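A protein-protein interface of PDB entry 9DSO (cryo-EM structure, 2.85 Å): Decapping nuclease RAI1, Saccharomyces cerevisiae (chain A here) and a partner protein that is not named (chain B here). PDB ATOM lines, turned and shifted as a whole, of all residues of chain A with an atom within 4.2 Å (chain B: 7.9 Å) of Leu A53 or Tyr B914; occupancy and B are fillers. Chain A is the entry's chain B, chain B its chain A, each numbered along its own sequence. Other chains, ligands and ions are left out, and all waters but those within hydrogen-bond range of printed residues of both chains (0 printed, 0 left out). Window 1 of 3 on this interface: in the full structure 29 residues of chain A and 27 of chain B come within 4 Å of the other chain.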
ATOM      1  N   TYR A  46     -11.672   4.403  12.788  1.00  0.00           N
ATOM      2  CA  TYR A  46     -11.122   5.619  12.211  1.00  0.00           C
ATOM      3  C   TYR A  46     -11.910   6.831  12.679  1.00  0.00           C
ATOM      4  O   TYR A  46     -13.143   6.827  12.674  1.00  0.00           O
ATOM      5  CB  TYR A  46     -11.130   5.542  10.687  1.00  0.00           C
ATOM      6  CG  TYR A  46     -10.392   6.679  10.027  1.00  0.00           C
ATOM      7  CD1 TYR A  46      -9.010   6.708  10.001  1.00  0.00           C
ATOM      8  CD2 TYR A  46     -11.076   7.728   9.439  1.00  0.00           C
ATOM      9  CE1 TYR A  46      -8.331   7.741   9.407  1.00  0.00           C
ATOM     10  CE2 TYR A  46     -10.404   8.769   8.842  1.00  0.00           C
ATOM     11  CZ  TYR A  46      -9.033   8.769   8.828  1.00  0.00           C
ATOM     12  OH  TYR A  46      -8.360   9.805   8.234  1.00  0.00           O
ATOM     13  N   LEU A  48     -10.759  11.000  12.135  1.00  0.00           N
ATOM     14  CA  LEU A  48      -9.810  12.093  11.929  1.00  0.00           C
ATOM     15  C   LEU A  48     -10.496  13.150  11.086  1.00  0.00           C
ATOM     16  O   LEU A  48     -10.504  13.074   9.850  1.00  0.00           O
ATOM     17  CB  LEU A  48      -8.523  11.612  11.265  1.00  0.00           C
ATOM     18  CG  LEU A  48      -7.372  12.613  11.184  1.00  0.00           C
ATOM     19  CD1 LEU A  48      -6.837  12.922  12.556  1.00  0.00           C
ATOM     20  CD2 LEU A  48      -6.275  12.079  10.294  1.00  0.00           C
ATOM     21  N   PRO A  49     -11.101  14.152  11.721  1.00  0.00           N
ATOM     22  CA  PRO A  49     -11.809  15.181  10.960  1.00  0.00           C
ATOM     23  C   PRO A  49     -10.856  15.990  10.098  1.00  0.00           C
ATOM     24  O   PRO A  49      -9.671  16.126  10.404  1.00  0.00           O
ATOM     25  CB  PRO A  49     -12.451  16.050  12.046  1.00  0.00           C
ATOM     26  CG  PRO A  49     -12.439  15.216  13.267  1.00  0.00           C
ATOM     27  CD  PRO A  49     -11.231  14.356  13.170  1.00  0.00           C
ATOM     28  N   ASP A  50     -11.394  16.522   9.000  1.00  0.00           N
ATOM     29  CA  ASP A  50     -10.595  17.357   8.112  1.00  0.00           C
ATOM     30  C   ASP A  50     -10.056  18.582   8.837  1.00  0.00           C
ATOM     31  O   ASP A  50      -8.914  18.993   8.601  1.00  0.00           O
ATOM     32  CB  ASP A  50     -11.430  17.757   6.897  1.00  0.00           C
ATOM     33  CG  ASP A  50     -10.776  18.831   6.064  1.00  0.00           C
ATOM     34  OD1 ASP A  50      -9.755  18.541   5.411  1.00  0.00           O
ATOM     35  OD2 ASP A  50     -11.294  19.965   6.043  1.00  0.00           O
ATOM     36  N   ALA A  51     -10.845  19.150   9.752  1.00  0.00           N
ATOM     37  CA  ALA A  51     -10.421  20.324  10.507  1.00  0.00           C
ATOM     38  C   ALA A  51      -9.185  20.060  11.354  1.00  0.00           C
ATOM     39  O   ALA A  51      -8.519  21.014  11.767  1.00  0.00           O
ATOM     40  CB  ALA A  51     -11.561  20.809  11.397  1.00  0.00           C
ATOM     41  N   GLU A  52      -8.868  18.796  11.626  1.00  0.00           N
ATOM     42  CA  GLU A  52      -7.676  18.460  12.390  1.00  0.00           C
ATOM     43  C   GLU A  52      -6.405  18.478  11.557  1.00  0.00           C
ATOM     44  O   GLU A  52      -5.313  18.463  12.132  1.00  0.00           O
ATOM     45  CB  GLU A  52      -7.832  17.086  13.039  1.00  0.00           C
ATOM     46  CG  GLU A  52      -8.762  17.087  14.228  1.00  0.00           C
ATOM     47  CD  GLU A  52      -8.610  15.856  15.082  1.00  0.00           C
ATOM     48  OE1 GLU A  52      -7.761  15.011  14.748  1.00  0.00           O
ATOM     49  OE2 GLU A  52      -9.341  15.730  16.084  1.00  0.00           O
ATOM     50  N   LEU A  53      -6.506  18.506  10.227  1.00  0.00           N
ATOM     51  CA  LEU A  53      -5.291  18.537   9.423  1.00  0.00           C
ATOM     52  C   LEU A  53      -4.609  19.894   9.481  1.00  0.00           C
ATOM     53  O   LEU A  53      -3.454  20.012   9.064  1.00  0.00           O
ATOM     54  CB  LEU A  53      -5.596  18.161   7.972  1.00  0.00           C
ATOM     55  CG  LEU A  53      -6.470  16.930   7.726  1.00  0.00           C
ATOM     56  CD1 LEU A  53      -6.505  16.599   6.251  1.00  0.00           C
ATOM     57  CD2 LEU A  53      -5.991  15.736   8.525  1.00  0.00           C
ATOM     58  N   ASP A  54      -5.296  20.913   9.992  1.00  0.00           N
ATOM     59  CA  ASP A  54      -4.743  22.253  10.134  1.00  0.00           C
ATOM     60  C   ASP A  54      -4.190  22.523  11.526  1.00  0.00           C
ATOM     61  O   ASP A  54      -3.779  23.653  11.803  1.00  0.00           O
ATOM     62  CB  ASP A  54      -5.809  23.299   9.800  1.00  0.00           C
ATOM     63  CG  ASP A  54      -6.166  23.318   8.330  1.00  0.00           C
ATOM     64  OD1 ASP A  54      -5.288  23.005   7.501  1.00  0.00           O
ATOM     65  OD2 ASP A  54      -7.325  23.644   8.003  1.00  0.00           O
ATOM     66  N   ARG A  55      -4.172  21.525  12.404  1.00  0.00           N
ATOM     67  CA  ARG A  55      -3.664  21.686  13.759  1.00  0.00           C
ATOM     68  C   ARG A  55      -2.165  21.446  13.867  1.00  0.00           C
ATOM     69  O   ARG A  55      -1.627  21.514  14.976  1.00  0.00           O
ATOM     70  CB  ARG A  55      -4.400  20.746  14.717  1.00  0.00           C
ATOM     71  CG  ARG A  55      -5.908  20.861  14.655  1.00  0.00           C
ATOM     72  CD  ARG A  55      -6.552  20.440  15.964  1.00  0.00           C
ATOM     73  NE  ARG A  55      -7.990  20.243  15.828  1.00  0.00           N
ATOM     74  CZ  ARG A  55      -8.882  21.221  15.758  1.00  0.00           C
ATOM     75  NH1 ARG A  55      -8.519  22.492  15.803  1.00  0.00           N
ATOM     76  NH2 ARG A  55     -10.170  20.917  15.639  1.00  0.00           N
ATOM     77  N   LEU A 287       2.191  16.438  10.223  1.00  0.00           N
ATOM     78  CA  LEU A 287       1.186  15.954   9.286  1.00  0.00           C
ATOM     79  C   LEU A 287       0.652  17.106   8.442  1.00  0.00           C
ATOM     80  O   LEU A 287      -0.093  17.955   8.940  1.00  0.00           O
ATOM     81  CB  LEU A 287       0.047  15.271  10.033  1.00  0.00           C
ATOM     82  CG  LEU A 287      -1.014  14.627   9.141  1.00  0.00           C
ATOM     83  CD1 LEU A 287      -0.550  13.268   8.659  1.00  0.00           C
ATOM     84  CD2 LEU A 287      -2.343  14.519   9.867  1.00  0.00           C
ATOM     85  N   LYS A 288       1.030  17.128   7.164  1.00  0.00           N
ATOM     86  CA  LYS A 288       0.536  18.124   6.222  1.00  0.00           C
ATOM     87  C   LYS A 288      -0.884  17.838   5.749  1.00  0.00           C
ATOM     88  O   LYS A 288      -1.734  18.731   5.782  1.00  0.00           O
ATOM     89  CB  LYS A 288       1.478  18.225   5.018  1.00  0.00           C
ATOM     90  CG  LYS A 288       2.906  18.649   5.326  1.00  0.00           C
ATOM     91  CD  LYS A 288       2.990  20.126   5.724  1.00  0.00           C
ATOM     92  CE  LYS A 288       2.932  20.360   7.224  1.00  0.00           C
ATOM     93  NZ  LYS A 288       3.123  21.798   7.562  1.00  0.00           N
ATOM     94  N   VAL A 290      -4.060  14.569   4.457  1.00  0.00           N
ATOM     95  CA  VAL A 290      -4.547  13.197   4.376  1.00  0.00           C
ATOM     96  C   VAL A 290      -5.351  13.055   3.090  1.00  0.00           C
ATOM     97  O   VAL A 290      -6.147  13.937   2.750  1.00  0.00           O
ATOM     98  CB  VAL A 290      -5.403  12.813   5.600  1.00  0.00           C
ATOM     99  CG1 VAL A 290      -6.126  11.510   5.355  1.00  0.00           C
ATOM    100  CG2 VAL A 290      -4.547  12.710   6.841  1.00  0.00           C
ATOM    101  N   GLU A 292      -7.523  10.052   0.504  1.00  0.00           N
ATOM    102  CA  GLU A 292      -8.217   8.772   0.509  1.00  0.00           C
ATOM    103  C   GLU A 292      -8.288   8.211  -0.904  1.00  0.00           C
ATOM    104  O   GLU A 292      -8.638   8.926  -1.847  1.00  0.00           O
ATOM    105  CB  GLU A 292      -9.623   8.917   1.089  1.00  0.00           C
ATOM    106  CG  GLU A 292      -9.672   9.745   2.356  1.00  0.00           C
ATOM    107  CD  GLU A 292     -11.050   9.798   2.973  1.00  0.00           C
ATOM    108  OE1 GLU A 292     -12.022  10.080   2.243  1.00  0.00           O
ATOM    109  OE2 GLU A 292     -11.159   9.564   4.193  1.00  0.00           O
ATOM    110  N   ASN B 863     -17.630  11.010  11.454  1.00  0.00           N
ATOM    111  CA  ASN B 863     -16.668  10.512  10.483  1.00  0.00           C
ATOM    112  C   ASN B 863     -17.341  10.260   9.140  1.00  0.00           C
ATOM    113  O   ASN B 863     -18.428   9.681   9.070  1.00  0.00           O
ATOM    114  CB  ASN B 863     -16.018   9.226  10.996  1.00  0.00           C
ATOM    115  CG  ASN B 863     -14.990   8.666  10.036  1.00  0.00           C
ATOM    116  OD1 ASN B 863     -15.073   7.512   9.627  1.00  0.00           O
ATOM    117  ND2 ASN B 863     -14.009   9.481   9.678  1.00  0.00           N
ATOM    118  N   GLY B 864     -16.684  10.690   8.069  1.00  0.00           N
ATOM    119  CA  GLY B 864     -17.205  10.499   6.732  1.00  0.00           C
ATOM    120  C   GLY B 864     -18.051  11.626   6.195  1.00  0.00           C
ATOM    121  O   GLY B 864     -18.737  11.433   5.187  1.00  0.00           O
ATOM    122  N   PHE B 865     -18.018  12.800   6.816  1.00  0.00           N
ATOM    123  CA  PHE B 865     -18.878  13.906   6.419  1.00  0.00           C
ATOM    124  C   PHE B 865     -18.228  14.660   5.264  1.00  0.00           C
ATOM    125  O   PHE B 865     -17.142  15.227   5.420  1.00  0.00           O
ATOM    126  CB  PHE B 865     -19.141  14.836   7.604  1.00  0.00           C
ATOM    127  CG  PHE B 865     -19.567  16.221   7.203  1.00  0.00           C
ATOM    128  CD1 PHE B 865     -20.860  16.467   6.784  1.00  0.00           C
ATOM    129  CD2 PHE B 865     -18.676  17.275   7.240  1.00  0.00           C
ATOM    130  CE1 PHE B 865     -21.251  17.729   6.407  1.00  0.00           C
ATOM    131  CE2 PHE B 865     -19.066  18.536   6.863  1.00  0.00           C
ATOM    132  CZ  PHE B 865     -20.353  18.760   6.444  1.00  0.00           C
ATOM    133  N   ILE B 866     -18.885  14.661   4.111  1.00  0.00           N
ATOM    134  CA  ILE B 866     -18.434  15.405   2.939  1.00  0.00           C
ATOM    135  C   ILE B 866     -19.225  16.707   2.882  1.00  0.00           C
ATOM    136  O   ILE B 866     -20.458  16.660   2.765  1.00  0.00           O
ATOM    137  CB  ILE B 866     -18.613  14.601   1.641  1.00  0.00           C
ATOM    138  CG1 ILE B 866     -17.769  13.330   1.650  1.00  0.00           C
ATOM    139  CG2 ILE B 866     -18.242  15.444   0.442  1.00  0.00           C
ATOM    140  CD1 ILE B 866     -18.532  12.085   2.006  1.00  0.00           C
ATOM    141  N   PRO B 867     -18.580  17.866   2.966  1.00  0.00           N
ATOM    142  CA  PRO B 867     -19.324  19.127   2.938  1.00  0.00           C
ATOM    143  C   PRO B 867     -19.930  19.401   1.570  1.00  0.00           C
ATOM    144  O   PRO B 867     -19.476  18.901   0.540  1.00  0.00           O
ATOM    145  CB  PRO B 867     -18.262  20.170   3.293  1.00  0.00           C
ATOM    146  CG  PRO B 867     -16.989  19.558   2.878  1.00  0.00           C
ATOM    147  CD  PRO B 867     -17.132  18.085   3.104  1.00  0.00           C
ATOM    148  N   ILE B 911     -16.602  12.742  -3.081  1.00  0.00           N
ATOM    149  CA  ILE B 911     -16.596  11.415  -2.478  1.00  0.00           C
ATOM    150  C   ILE B 911     -15.738  11.438  -1.219  1.00  0.00           C
ATOM    151  O   ILE B 911     -15.931  10.630  -0.305  1.00  0.00           O
ATOM    152  CB  ILE B 911     -16.088  10.360  -3.479  1.00  0.00           C
ATOM    153  CG1 ILE B 911     -16.908  10.405  -4.767  1.00  0.00           C
ATOM    154  CG2 ILE B 911     -16.162   8.966  -2.886  1.00  0.00           C
ATOM    155  CD1 ILE B 911     -18.341   9.951  -4.597  1.00  0.00           C
ATOM    156  N   THR B 912     -14.794  12.370  -1.155  1.00  0.00           N
ATOM    157  CA  THR B 912     -13.820  12.412  -0.077  1.00  0.00           C
ATOM    158  C   THR B 912     -14.173  13.493   0.937  1.00  0.00           C
ATOM    159  O   THR B 912     -14.674  14.565   0.588  1.00  0.00           O
ATOM    160  CB  THR B 912     -12.413  12.651  -0.627  1.00  0.00           C
ATOM    161  OG1 THR B 912     -11.476  12.714   0.452  1.00  0.00           O
ATOM    162  CG2 THR B 912     -12.359  13.947  -1.410  1.00  0.00           C
ATOM    163  N   GLN B 913     -13.911  13.192   2.209  1.00  0.00           N
ATOM    164  CA  GLN B 913     -14.136  14.126   3.302  1.00  0.00           C
ATOM    165  C   GLN B 913     -12.995  15.108   3.507  1.00  0.00           C
ATOM    166  O   GLN B 913     -13.143  16.042   4.300  1.00  0.00           O
ATOM    167  CB  GLN B 913     -14.372  13.368   4.608  1.00  0.00           C
ATOM    168  CG  GLN B 913     -13.174  12.578   5.079  1.00  0.00           C
ATOM    169  CD  GLN B 913     -13.449  11.797   6.341  1.00  0.00           C
ATOM    170  OE1 GLN B 913     -14.526  11.886   6.911  1.00  0.00           O
ATOM    171  NE2 GLN B 913     -12.485  10.997   6.765  1.00  0.00           N
ATOM    172  N   TYR B 914     -11.872  14.929   2.821  1.00  0.00           N
ATOM    173  CA  TYR B 914     -10.704  15.781   2.978  1.00  0.00           C
ATOM    174  C   TYR B 914     -10.540  16.655   1.745  1.00  0.00           C
ATOM    175  O   TYR B 914     -10.510  16.149   0.621  1.00  0.00           O
ATOM    176  CB  TYR B 914      -9.447  14.942   3.202  1.00  0.00           C
ATOM    177  CG  TYR B 914      -9.484  14.120   4.463  1.00  0.00           C
ATOM    178  CD1 TYR B 914      -9.401  14.724   5.704  1.00  0.00           C
ATOM    179  CD2 TYR B 914      -9.601  12.745   4.413  1.00  0.00           C
ATOM    180  CE1 TYR B 914      -9.437  13.987   6.855  1.00  0.00           C
ATOM    181  CE2 TYR B 914      -9.637  11.999   5.564  1.00  0.00           C
ATOM    182  CZ  TYR B 914      -9.556  12.627   6.783  1.00  0.00           C
ATOM    183  OH  TYR B 914      -9.590  11.887   7.937  1.00  0.00           O
ATOM    184  N   LYS B 915     -10.441  17.955   1.957  1.00  0.00           N
ATOM    185  CA  LYS B 915     -10.247  18.873   0.849  1.00  0.00           C
ATOM    186  C   LYS B 915      -8.791  18.849   0.385  1.00  0.00           C
ATOM    187  O   LYS B 915      -7.893  18.518   1.162  1.00  0.00           O
ATOM    188  CB  LYS B 915     -10.643  20.288   1.256  1.00  0.00           C
ATOM    189  CG  LYS B 915      -9.843  20.851   2.405  1.00  0.00           C
ATOM    190  CD  LYS B 915     -10.312  22.243   2.773  1.00  0.00           C
ATOM    191  CE  LYS B 915      -9.717  23.285   1.850  1.00  0.00           C
ATOM    192  NZ  LYS B 915      -8.237  23.375   1.982  1.00  0.00           N
ATOM    193  N   PRO B 916      -8.538  19.168  -0.884  1.00  0.00           N
ATOM    194  CA  PRO B 916      -7.154  19.202  -1.367  1.00  0.00           C
ATOM    195  C   PRO B 916      -6.325  20.224  -0.607  1.00  0.00           C
ATOM    196  O   PRO B 916      -6.800  21.307  -0.259  1.00  0.00           O
ATOM    197  CB  PRO B 916      -7.302  19.582  -2.842  1.00  0.00           C
ATOM    198  CG  PRO B 916      -8.676  19.167  -3.197  1.00  0.00           C
ATOM    199  CD  PRO B 916      -9.501  19.388  -1.974  1.00  0.00           C
ATOM    200  N   ARG B 917      -5.069  19.870  -0.358  1.00  0.00           N
ATOM    201  CA  ARG B 917      -4.181  20.688   0.450  1.00  0.00           C
ATOM    202  C   ARG B 917      -2.752  20.407   0.018  1.00  0.00           C
ATOM    203  O   ARG B 917      -2.383  19.252  -0.196  1.00  0.00           O
ATOM    204  CB  ARG B 917      -4.378  20.391   1.939  1.00  0.00           C
ATOM    205  CG  ARG B 917      -3.787  21.419   2.870  1.00  0.00           C
ATOM    206  CD  ARG B 917      -4.171  21.137   4.314  1.00  0.00           C
ATOM    207  NE  ARG B 917      -5.563  21.456   4.610  1.00  0.00           N
ATOM    208  CZ  ARG B 917      -6.537  20.561   4.691  1.00  0.00           C
ATOM    209  NH1 ARG B 917      -6.322  19.282   4.444  1.00  0.00           N
ATOM    210  NH2 ARG B 917      -7.757  20.960   5.035  1.00  0.00           N
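NH2 of Arg B917 lies within salt-bridge range of OD1 of Asp A50 (3.2 Å).
OH of Tyr B914 sits at hydrogen-bond distance from O of Leu A48.
The side-chain amide nitrogen of Gln B913 lies within hydrogen-bond range of the side-chain carboxylate of Glu A292 (3.2 Å).
OH of Tyr B914 lies within hydrogen-bond range of OH of Tyr A46 (2.4 Å).
The side-chain carboxylate (OD1) of Asp A54 lies within salt-bridge range of the guanidinium group (NE) of Arg B917 (3.3 Å).
The side-chain hydroxyl (OG1) of Thr B912 is in hydrogen-bond range of the side-chain carboxylate (OE1) of Glu A292, at 3.2 Å.
NE2 of Gln B913 is in hydrogen-bond range of OH of Tyr B914 (3.2 Å).
OE1 of Gln B913 lies within hydrogen-bond range of N of Gly B864 (2.7 Å).
The backbone NH of Tyr B914 lies within hydrogen-bond range of the side-chain hydroxyl of Thr B912.
CD2 of Tyr A46 touches ND2 of Asn B863 (3.4 Å).
Tyr A46 touches Gln B913.
Gln B913 touches Asp A50 (O to CB, 3.6 Å).
CA of Asp A50 touches CD1 of Tyr B914 (3.8 Å).
Asp A50 touches Lys B915.
Leu A53 touches Tyr B914.
CD1 of Leu A53 touches NH1 of Arg B917 (3.2 Å).
Lys A288 touches Arg B917 (O to CD, 3.7 Å).
O of Val A290 touches CB of Tyr B914 (3.5 Å).
Tyr B914 touches Glu A292 (CE2 to OE2, 3.2 Å).
Of the printed residues of chain B, Leu A48 touches Tyr B914.
Of chain B, only Tyr B914 and Arg B917 come within 4 Å of Leu A53.
Of the printed residues of chain B, Asp A54 touches Arg B917.
Arg A55 touches none of the printed residues of chain B.
Of the printed residues of chain B, Val A290 touches Tyr B914 (3.5 Å).
Phe B865 touches none of the printed residues of chain A.
Printed residues of chain A within 4 Å of Tyr B914: Tyr A46 (2.4 Å), Leu A48 (2.4 Å), Asp A50 (3.8 Å), Leu A53 (3.5 Å), Val A290 (3.5 Å) and Glu A292 (3.2 Å).
The nearest residue of chain B that does not touch Leu A53 is Lys B915 (5.6 Å).
The nearest residue of chain A that does not touch Tyr B914 is Pro A49 (4.1 Å).
Printed residues of chain B that touch a printed residue of chain A: Asn B863, Thr B912, Gln B913, Tyr B914, Lys B915 and Arg B917.
Hydrophobic or aromatic side chains of chain B that line the printed part of chain A: Tyr B914.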
